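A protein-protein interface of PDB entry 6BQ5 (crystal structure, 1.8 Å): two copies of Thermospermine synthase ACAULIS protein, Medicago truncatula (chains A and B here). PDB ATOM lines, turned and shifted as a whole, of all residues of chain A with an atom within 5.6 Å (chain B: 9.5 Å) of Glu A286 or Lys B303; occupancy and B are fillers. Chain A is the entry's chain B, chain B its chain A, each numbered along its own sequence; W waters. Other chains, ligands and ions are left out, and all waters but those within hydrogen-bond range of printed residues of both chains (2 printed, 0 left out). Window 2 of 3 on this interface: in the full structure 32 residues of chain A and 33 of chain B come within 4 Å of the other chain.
Of the printed residues of chain A, Ser B302 touches Tyr A289 and Thr A294.
Printed residues of chain A within 4 Å of Arg B306: Asp A291 and Thr A294.
Printed residues of chain B within 4 Å of Thr A294: Ser B302, Lys B303 and Arg B306.
Asn B311 touches none of the printed residues of chain A.
The nearest residue of chain B that does not touch Glu A286 is Asn B307 (8.5 Å).
The nearest printed residue of chain B that does not touch Asp A291 is Ser B302 (4.8 Å).
The side-chain carboxylate of Glu A89 lies within hydrogen-bond range of the backbone NH of Tyr A289, 2.8 Å away.
The side-chain amide oxygen of Asn B310 sits close to the backbone carbonyl oxygen of Arg B306, at 3.0 Å.
The backbone carbonyl oxygen (O) of Leu B301 is in hydrogen-bond range of the guanidinium group (NH2) of Arg B306.
The side-chain carboxylate of Asp A291 sits at hydrogen-bond distance from the side-chain hydroxyl of Thr A294, at 2.6 Å.
ND2 of Asn A287 sits at hydrogen-bond distance from O of Leu A290, at 3.3 Å.
OD1 of Asn A287 sits at hydrogen-bond distance from NH1 of Arg A121 (3.0 Å).
CB of Ser B302 touches CE1 of Tyr A289 (3.9 Å).
Tyr A289 touches Lys B303.
Asp A291 touches Lys B303 (OD2 to CB, 3.7 Å).
CA of Ser B302 touches OG1 of Thr A294 (3.3 Å).
No position is printed for both chains.
NZ of Lys B303 lies within salt-bridge range of OE2 of Glu A286 (2.8 Å).
OG1 of Thr A294 lies within hydrogen-bond range of NH2 of Arg B306, at 3.4 Å.
N of Lys B303 sits at hydrogen-bond distance from OG1 of Thr A294, at 2.8 Å.
The side-chain amino group of Lys B303 sits at hydrogen-bond distance from the backbone carbonyl oxygen of Asn A287, 2.7 Å away.
The side-chain carboxylate (OD2) of Asp A291 lies within salt-bridge range of the guanidinium group (NH1) of Arg B306, 2.8 Å away.
Of the 14 printed residues of chain B, 3 touch a printed residue of chain A.
Among the printed residues, Asp or Glu carboxylates within 4 Å of a Lys or Arg side-chain nitrogen of the other chain: Glu A286 with Lys B303 and Asp A291 with Arg B306.
Water W2 lies within hydrogen-bond range of the backbone carbonyl oxygen (O) of Leu A290 (2.7 Å) and the side-chain amino group (NZ) of Lys B303 (3.1 Å).
Water W1 lies within hydrogen-bond range of the backbone carbonyl oxygen (O) of Tyr A289 (2.7 Å), the backbone NH (N) of Ala B304 (2.8 Å), the side-chain hydroxyl (OG) of Ser B302 (3.0 Å) and the backbone NH (N) of Lys B303 (3.2 Å).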
ATOM      1  N   GLU A  89      20.369 -11.382  13.202  1.00  0.00           N
ATOM      2  CA  GLU A  89      18.904 -11.208  13.099  1.00  0.00           C
ATOM      3  C   GLU A  89      18.566 -10.328  11.886  1.00  0.00           C
ATOM      4  O   GLU A  89      17.626 -10.659  11.139  1.00  0.00           O
ATOM      5  CB  GLU A  89      18.302 -10.556  14.339  1.00  0.00           C
ATOM      6  CG  GLU A  89      18.183 -11.519  15.525  1.00  0.00           C
ATOM      7  CD  GLU A  89      17.387 -10.973  16.675  1.00  0.00           C
ATOM      8  OE1 GLU A  89      16.732  -9.855  16.550  1.00  0.00           O
ATOM      9  OE2 GLU A  89      17.485 -11.579  17.771  1.00  0.00           O
ATOM     10  N   ARG A 121      15.967 -21.176  13.705  1.00  0.00           N
ATOM     11  CA  ARG A 121      14.848 -20.784  14.570  1.00  0.00           C
ATOM     12  C   ARG A 121      13.527 -20.744  13.812  1.00  0.00           C
ATOM     13  O   ARG A 121      12.496 -20.753  14.447  1.00  0.00           O
ATOM     14  CB  ARG A 121      15.106 -19.425  15.218  1.00  0.00           C
ATOM     15  CG  ARG A 121      16.244 -19.438  16.239  1.00  0.00           C
ATOM     16  CD  ARG A 121      16.596 -18.026  16.722  1.00  0.00           C
ATOM     17  NE  ARG A 121      15.436 -17.484  17.372  1.00  0.00           N
ATOM     18  CZ  ARG A 121      15.141 -16.182  17.432  1.00  0.00           C
ATOM     19  NH1 ARG A 121      15.949 -15.280  16.868  1.00  0.00           N
ATOM     20  NH2 ARG A 121      14.040 -15.788  18.022  1.00  0.00           N
ATOM     21  N   ARG A 280       5.943 -14.228  15.401  1.00  0.00           N
ATOM     22  CA  ARG A 280       5.344 -14.966  16.510  1.00  0.00           C
ATOM     23  C   ARG A 280       4.886 -16.352  16.080  1.00  0.00           C
ATOM     24  O   ARG A 280       5.031 -17.299  16.860  1.00  0.00           O
ATOM     25  CB  ARG A 280       4.175 -14.180  17.070  1.00  0.00           C
ATOM     26  CG  ARG A 280       3.690 -14.672  18.426  1.00  0.00           C
ATOM     27  CD  ARG A 280       2.610 -13.748  18.947  1.00  0.00           C
ATOM     28  NE  ARG A 280       3.026 -12.973  20.132  1.00  0.00           N
ATOM     29  CZ  ARG A 280       3.651 -11.784  20.090  1.00  0.00           C
ATOM     30  NH1 ARG A 280       3.954 -11.213  18.905  1.00  0.00           N
ATOM     31  NH2 ARG A 280       3.955 -11.151  21.228  1.00  0.00           N
ATOM     32  N   ILE A 284      10.888 -19.627  16.504  1.00  0.00           N
ATOM     33  CA  ILE A 284      11.004 -20.040  17.900  1.00  0.00           C
ATOM     34  C   ILE A 284      11.700 -18.946  18.711  1.00  0.00           C
ATOM     35  O   ILE A 284      12.657 -18.341  18.220  1.00  0.00           O
ATOM     36  CB  ILE A 284      11.809 -21.349  18.006  1.00  0.00           C
ATOM     37  CG1 ILE A 284      11.030 -22.492  17.329  1.00  0.00           C
ATOM     38  CG2 ILE A 284      12.077 -21.698  19.480  1.00  0.00           C
ATOM     39  CD1 ILE A 284      11.765 -23.833  17.351  1.00  0.00           C
ATOM     40  N   GLU A 285      11.245 -18.723  19.950  1.00  0.00           N
ATOM     41  CA  GLU A 285      11.767 -17.663  20.839  1.00  0.00           C
ATOM     42  C   GLU A 285      11.540 -16.201  20.326  1.00  0.00           C
ATOM     43  O   GLU A 285      11.230 -15.950  19.165  1.00  0.00           O
ATOM     44  CB  GLU A 285      13.265 -17.907  21.169  1.00  0.00           C
ATOM     45  CG  GLU A 285      13.576 -19.266  21.835  1.00  0.00           C
ATOM     46  CD  GLU A 285      14.921 -19.930  21.456  1.00  0.00           C
ATOM     47  OE1 GLU A 285      15.514 -19.580  20.376  1.00  0.00           O
ATOM     48  OE2 GLU A 285      15.363 -20.829  22.211  1.00  0.00           O
ATOM     49  N   GLU A 286      11.707 -15.226  21.200  1.00  0.00           N
ATOM     50  CA  GLU A 286      11.587 -13.842  20.824  1.00  0.00           C
ATOM     51  C   GLU A 286      12.916 -13.395  20.207  1.00  0.00           C
ATOM     52  O   GLU A 286      13.998 -13.701  20.714  1.00  0.00           O
ATOM     53  CB  GLU A 286      11.277 -12.950  22.031  1.00  0.00           C
ATOM     54  CG  GLU A 286       9.868 -13.054  22.573  1.00  0.00           C
ATOM     55  CD  GLU A 286       8.858 -12.272  21.753  1.00  0.00           C
ATOM     56  OE1 GLU A 286       7.814 -12.868  21.374  1.00  0.00           O
ATOM     57  OE2 GLU A 286       9.090 -11.041  21.503  1.00  0.00           O
ATOM     58  N   ASN A 287      12.841 -12.688  19.096  1.00  0.00           N
ATOM     59  CA  ASN A 287      13.995 -11.912  18.629  1.00  0.00           C
ATOM     60  C   ASN A 287      14.387 -10.890  19.669  1.00  0.00           C
ATOM     61  O   ASN A 287      13.524 -10.356  20.385  1.00  0.00           O
ATOM     62  CB  ASN A 287      13.667 -11.179  17.351  1.00  0.00           C
ATOM     63  CG  ASN A 287      13.532 -12.084  16.164  1.00  0.00           C
ATOM     64  OD1 ASN A 287      13.872 -13.249  16.205  1.00  0.00           O
ATOM     65  ND2 ASN A 287      13.050 -11.534  15.066  1.00  0.00           N
ATOM     66  N   ARG A 288      15.683 -10.585  19.743  1.00  0.00           N
ATOM     67  CA  ARG A 288      16.142  -9.577  20.678  1.00  0.00           C
ATOM     68  C   ARG A 288      16.326  -8.201  20.096  1.00  0.00           C
ATOM     69  O   ARG A 288      16.350  -7.197  20.845  1.00  0.00           O
ATOM     70  CB  ARG A 288      17.468  -9.980  21.278  1.00  0.00           C
ATOM     71  CG  ARG A 288      17.350 -11.120  22.265  1.00  0.00           C
ATOM     72  CD  ARG A 288      18.594 -11.127  23.135  1.00  0.00           C
ATOM     73  NE  ARG A 288      19.691 -11.892  22.566  1.00  0.00           N
ATOM     74  CZ  ARG A 288      20.984 -11.687  22.853  1.00  0.00           C
ATOM     75  NH1 ARG A 288      21.916 -12.492  22.343  1.00  0.00           N
ATOM     76  NH2 ARG A 288      21.351 -10.648  23.645  1.00  0.00           N
ATOM     77  N   TYR A 289      16.553  -8.144  18.791  1.00  0.00           N
ATOM     78  CA  TYR A 289      16.784  -6.882  18.114  1.00  0.00           C
ATOM     79  C   TYR A 289      15.564  -6.517  17.313  1.00  0.00           C
ATOM     80  O   TYR A 289      15.100  -5.397  17.397  1.00  0.00           O
ATOM     81  CB  TYR A 289      18.037  -6.916  17.220  1.00  0.00           C
ATOM     82  CG  TYR A 289      18.218  -5.598  16.549  1.00  0.00           C
ATOM     83  CD1 TYR A 289      18.535  -4.488  17.287  1.00  0.00           C
ATOM     84  CD2 TYR A 289      17.946  -5.435  15.169  1.00  0.00           C
ATOM     85  CE1 TYR A 289      18.605  -3.254  16.678  1.00  0.00           C
ATOM     86  CE2 TYR A 289      18.001  -4.181  14.576  1.00  0.00           C
ATOM     87  CZ  TYR A 289      18.318  -3.109  15.344  1.00  0.00           C
ATOM     88  OH  TYR A 289      18.387  -1.879  14.802  1.00  0.00           O
ATOM     89  N   LEU A 290      15.082  -7.452  16.490  1.00  0.00           N
ATOM     90  CA  LEU A 290      14.228  -7.090  15.397  1.00  0.00           C
ATOM     91  C   LEU A 290      12.750  -7.359  15.683  1.00  0.00           C
ATOM     92  O   LEU A 290      12.368  -8.483  15.994  1.00  0.00           O
ATOM     93  CB  LEU A 290      14.651  -7.859  14.174  1.00  0.00           C
ATOM     94  CG  LEU A 290      13.983  -7.434  12.876  1.00  0.00           C
ATOM     95  CD1 LEU A 290      14.664  -6.207  12.277  1.00  0.00           C
ATOM     96  CD2 LEU A 290      13.990  -8.604  11.890  1.00  0.00           C
ATOM     97  N   ASP A 291      11.916  -6.318  15.607  1.00  0.00           N
ATOM     98  CA  ASP A 291      10.478  -6.487  15.353  1.00  0.00           C
ATOM     99  C   ASP A 291      10.117  -5.811  14.035  1.00  0.00           C
ATOM    100  O   ASP A 291      11.005  -5.340  13.309  1.00  0.00           O
ATOM    101  CB  ASP A 291       9.623  -6.015  16.506  1.00  0.00           C
ATOM    102  CG  ASP A 291       9.734  -4.540  16.819  1.00  0.00           C
ATOM    103  OD1 ASP A 291      10.388  -3.778  16.067  1.00  0.00           O
ATOM    104  OD2 ASP A 291       9.169  -4.143  17.839  1.00  0.00           O
ATOM    105  N   THR A 294      11.042  -2.171  13.782  1.00  0.00           N
ATOM    106  CA  THR A 294      12.499  -2.056  13.631  1.00  0.00           C
ATOM    107  C   THR A 294      12.874  -2.231  12.170  1.00  0.00           C
ATOM    108  O   THR A 294      13.657  -1.471  11.614  1.00  0.00           O
ATOM    109  CB  THR A 294      13.236  -3.061  14.524  1.00  0.00           C
ATOM    110  OG1 THR A 294      12.798  -2.903  15.862  1.00  0.00           O
ATOM    111  CG2 THR A 294      14.729  -2.886  14.443  1.00  0.00           C
ATOM    112  N   ILE B 223      21.825   0.505  21.334  1.00  0.00           N
ATOM    113  CA  ILE B 223      21.147  -0.701  21.760  1.00  0.00           C
ATOM    114  C   ILE B 223      21.319  -1.068  23.257  1.00  0.00           C
ATOM    115  O   ILE B 223      20.374  -1.522  23.880  1.00  0.00           O
ATOM    116  CB  ILE B 223      21.487  -1.878  20.834  1.00  0.00           C
ATOM    117  CG1 ILE B 223      20.516  -3.075  21.024  1.00  0.00           C
ATOM    118  CG2 ILE B 223      22.930  -2.297  21.017  1.00  0.00           C
ATOM    119  CD1 ILE B 223      19.042  -2.692  20.960  1.00  0.00           C
ATOM    120  N   HIS B 226      21.354   3.150  25.613  1.00  0.00           N
ATOM    121  CA  HIS B 226      20.060   3.881  25.800  1.00  0.00           C
ATOM    122  C   HIS B 226      19.502   3.850  27.228  1.00  0.00           C
ATOM    123  O   HIS B 226      18.695   4.695  27.570  1.00  0.00           O
ATOM    124  CB  HIS B 226      18.964   3.406  24.839  1.00  0.00           C
ATOM    125  CG  HIS B 226      18.346   2.100  25.214  1.00  0.00           C
ATOM    126  ND1 HIS B 226      18.877   0.888  24.837  1.00  0.00           N
ATOM    127  CD2 HIS B 226      17.246   1.817  25.954  1.00  0.00           C
ATOM    128  CE1 HIS B 226      18.111  -0.092  25.309  1.00  0.00           C
ATOM    129  NE2 HIS B 226      17.111   0.439  25.978  1.00  0.00           N
ATOM    130  N   THR B 300      11.262   6.114  14.939  1.00  0.00           N
ATOM    131  CA  THR B 300      10.837   4.721  15.043  1.00  0.00           C
ATOM    132  C   THR B 300      12.001   3.951  15.640  1.00  0.00           C
ATOM    133  O   THR B 300      12.953   3.576  14.919  1.00  0.00           O
ATOM    134  CB  THR B 300      10.499   4.130  13.667  1.00  0.00           C
ATOM    135  OG1 THR B 300       9.633   5.041  12.947  1.00  0.00           O
ATOM    136  CG2 THR B 300       9.864   2.740  13.847  1.00  0.00           C
ATOM    137  N   LEU B 301      11.951   3.795  16.948  1.00  0.00           N
ATOM    138  CA  LEU B 301      13.020   3.157  17.698  1.00  0.00           C
ATOM    139  C   LEU B 301      12.968   1.648  17.526  1.00  0.00           C
ATOM    140  O   LEU B 301      11.929   1.123  17.102  1.00  0.00           O
ATOM    141  CB  LEU B 301      12.919   3.537  19.130  1.00  0.00           C
ATOM    142  CG  LEU B 301      12.911   5.069  19.339  1.00  0.00           C
ATOM    143  CD1 LEU B 301      12.715   5.390  20.775  1.00  0.00           C
ATOM    144  CD2 LEU B 301      14.216   5.677  18.824  1.00  0.00           C
ATOM    145  N   SER B 302      14.076   0.951  17.827  1.00  0.00           N
ATOM    146  CA  SER B 302      14.177  -0.469  17.650  1.00  0.00           C
ATOM    147  C   SER B 302      13.417  -1.146  18.770  1.00  0.00           C
ATOM    148  O   SER B 302      13.014  -0.497  19.742  1.00  0.00           O
ATOM    149  CB  SER B 302      15.644  -0.962  17.657  1.00  0.00           C
ATOM    150  OG  SER B 302      16.177  -0.873  18.991  1.00  0.00           O
ATOM    151  N   LYS B 303      13.234  -2.454  18.637  1.00  0.00           N
ATOM    152  CA  LYS B 303      12.449  -3.204  19.622  1.00  0.00           C
ATOM    153  C   LYS B 303      12.887  -2.981  21.060  1.00  0.00           C
ATOM    154  O   LYS B 303      12.025  -2.691  21.925  1.00  0.00           O
ATOM    155  CB  LYS B 303      12.495  -4.699  19.311  1.00  0.00           C
ATOM    156  CG  LYS B 303      11.647  -5.555  20.226  1.00  0.00           C
ATOM    157  CD  LYS B 303      11.780  -7.008  19.869  1.00  0.00           C
ATOM    158  CE  LYS B 303      10.918  -7.820  20.833  1.00  0.00           C
ATOM    159  NZ  LYS B 303      11.057  -9.233  20.520  1.00  0.00           N
ATOM    160  N   ALA B 304      14.181  -3.166  21.349  1.00  0.00           N
ATOM    161  CA  ALA B 304      14.632  -3.171  22.740  1.00  0.00           C
ATOM    162  C   ALA B 304      14.594  -1.768  23.307  1.00  0.00           C
ATOM    163  O   ALA B 304      14.305  -1.573  24.486  1.00  0.00           O
ATOM    164  CB  ALA B 304      16.016  -3.747  22.906  1.00  0.00           C
ATOM    165  N   VAL B 305      14.850  -0.789  22.457  1.00  0.00           N
ATOM    166  CA  VAL B 305      14.873   0.599  22.915  1.00  0.00           C
ATOM    167  C   VAL B 305      13.423   1.035  23.238  1.00  0.00           C
ATOM    168  O   VAL B 305      13.163   1.627  24.290  1.00  0.00           O
ATOM    169  CB  VAL B 305      15.534   1.515  21.846  1.00  0.00           C
ATOM    170  CG1 VAL B 305      15.457   2.973  22.251  1.00  0.00           C
ATOM    171  CG2 VAL B 305      16.986   1.159  21.640  1.00  0.00           C
ATOM    172  N   ARG B 306      12.477   0.746  22.347  1.00  0.00           N
ATOM    173  CA  ARG B 306      11.058   1.084  22.611  1.00  0.00           C
ATOM    174  C   ARG B 306      10.569   0.438  23.899  1.00  0.00           C
ATOM    175  O   ARG B 306       9.864   1.071  24.701  1.00  0.00           O
ATOM    176  CB  ARG B 306      10.137   0.622  21.489  1.00  0.00           C
ATOM    177  CG  ARG B 306       9.465   1.729  20.741  1.00  0.00           C
ATOM    178  CD  ARG B 306       8.600   1.179  19.603  1.00  0.00           C
ATOM    179  NE  ARG B 306       9.441   0.577  18.576  1.00  0.00           N
ATOM    180  CZ  ARG B 306       9.431  -0.713  18.251  1.00  0.00           C
ATOM    181  NH1 ARG B 306       8.519  -1.556  18.800  1.00  0.00           N
ATOM    182  NH2 ARG B 306      10.265  -1.161  17.353  1.00  0.00           N
ATOM    183  N   ASN B 307      10.924  -0.815  24.083  1.00  0.00           N
ATOM    184  CA  ASN B 307      10.517  -1.581  25.298  1.00  0.00           C
ATOM    185  C   ASN B 307      11.082  -0.904  26.558  1.00  0.00           C
ATOM    186  O   ASN B 307      10.342  -0.705  27.541  1.00  0.00           O
ATOM    187  CB  ASN B 307      10.993  -3.040  25.145  1.00  0.00           C
ATOM    188  CG  ASN B 307      10.688  -3.938  26.361  1.00  0.00           C
ATOM    189  OD1 ASN B 307       9.543  -4.312  26.600  1.00  0.00           O
ATOM    190  ND2 ASN B 307      11.727  -4.311  27.108  1.00  0.00           N
ATOM    191  N   SER B 308      12.368  -0.523  26.543  1.00  0.00           N
ATOM    192  CA  SER B 308      12.953   0.221  27.704  1.00  0.00           C
ATOM    193  C   SER B 308      12.207   1.513  27.980  1.00  0.00           C
ATOM    194  O   SER B 308      11.838   1.781  29.121  1.00  0.00           O
ATOM    195  CB  SER B 308      14.445   0.537  27.562  1.00  0.00           C
ATOM    196  OG  SER B 308      15.199  -0.630  27.466  1.00  0.00           O
ATOM    197  N   LEU B 309      11.997   2.306  26.939  1.00  0.00           N
ATOM    198  CA  LEU B 309      11.318   3.585  27.114  1.00  0.00           C
ATOM    199  C   LEU B 309       9.914   3.375  27.642  1.00  0.00           C
ATOM    200  O   LEU B 309       9.495   4.041  28.563  1.00  0.00           O
ATOM    201  CB  LEU B 309      11.305   4.414  25.800  1.00  0.00           C
ATOM    202  CG  LEU B 309      12.502   5.377  25.701  1.00  0.00           C
ATOM    203  CD1 LEU B 309      13.848   4.691  25.615  1.00  0.00           C
ATOM    204  CD2 LEU B 309      12.265   6.281  24.495  1.00  0.00           C
ATOM    205  N   ASN B 310       9.229   2.367  27.133  1.00  0.00           N
ATOM    206  CA  ASN B 310       7.843   2.155  27.502  1.00  0.00           C
ATOM    207  C   ASN B 310       7.678   1.500  28.877  1.00  0.00           C
ATOM    208  O   ASN B 310       6.661   1.755  29.543  1.00  0.00           O
ATOM    209  CB  ASN B 310       7.076   1.445  26.371  1.00  0.00           C
ATOM    210  CG  ASN B 310       6.894   2.365  25.136  1.00  0.00           C
ATOM    211  OD1 ASN B 310       7.074   1.937  23.980  1.00  0.00           O
ATOM    212  ND2 ASN B 310       6.537   3.651  25.386  1.00  0.00           N
ATOM    213  N   ASN B 311       8.681   0.770  29.342  1.00  0.00           N
ATOM    214  CA  ASN B 311       8.622   0.126  30.660  1.00  0.00           C
ATOM    215  C   ASN B 311       9.326   0.960  31.718  1.00  0.00           C
ATOM    216  O   ASN B 311       9.251   0.647  32.847  1.00  0.00           O
ATOM    217  CB  ASN B 311       9.228  -1.278  30.611  1.00  0.00           C
ATOM    218  CG  ASN B 311       8.437  -2.213  29.704  1.00  0.00           C
ATOM    219  OD1 ASN B 311       7.270  -1.954  29.430  1.00  0.00           O
ATOM    220  ND2 ASN B 311       9.066  -3.289  29.226  1.00  0.00           N
HETATM  221  O   HOH W   1      16.078  -3.834  19.382  1.00  0.00           O
HETATM  222  O   HOH W   2      10.323  -9.379  17.507  1.00  0.00           O
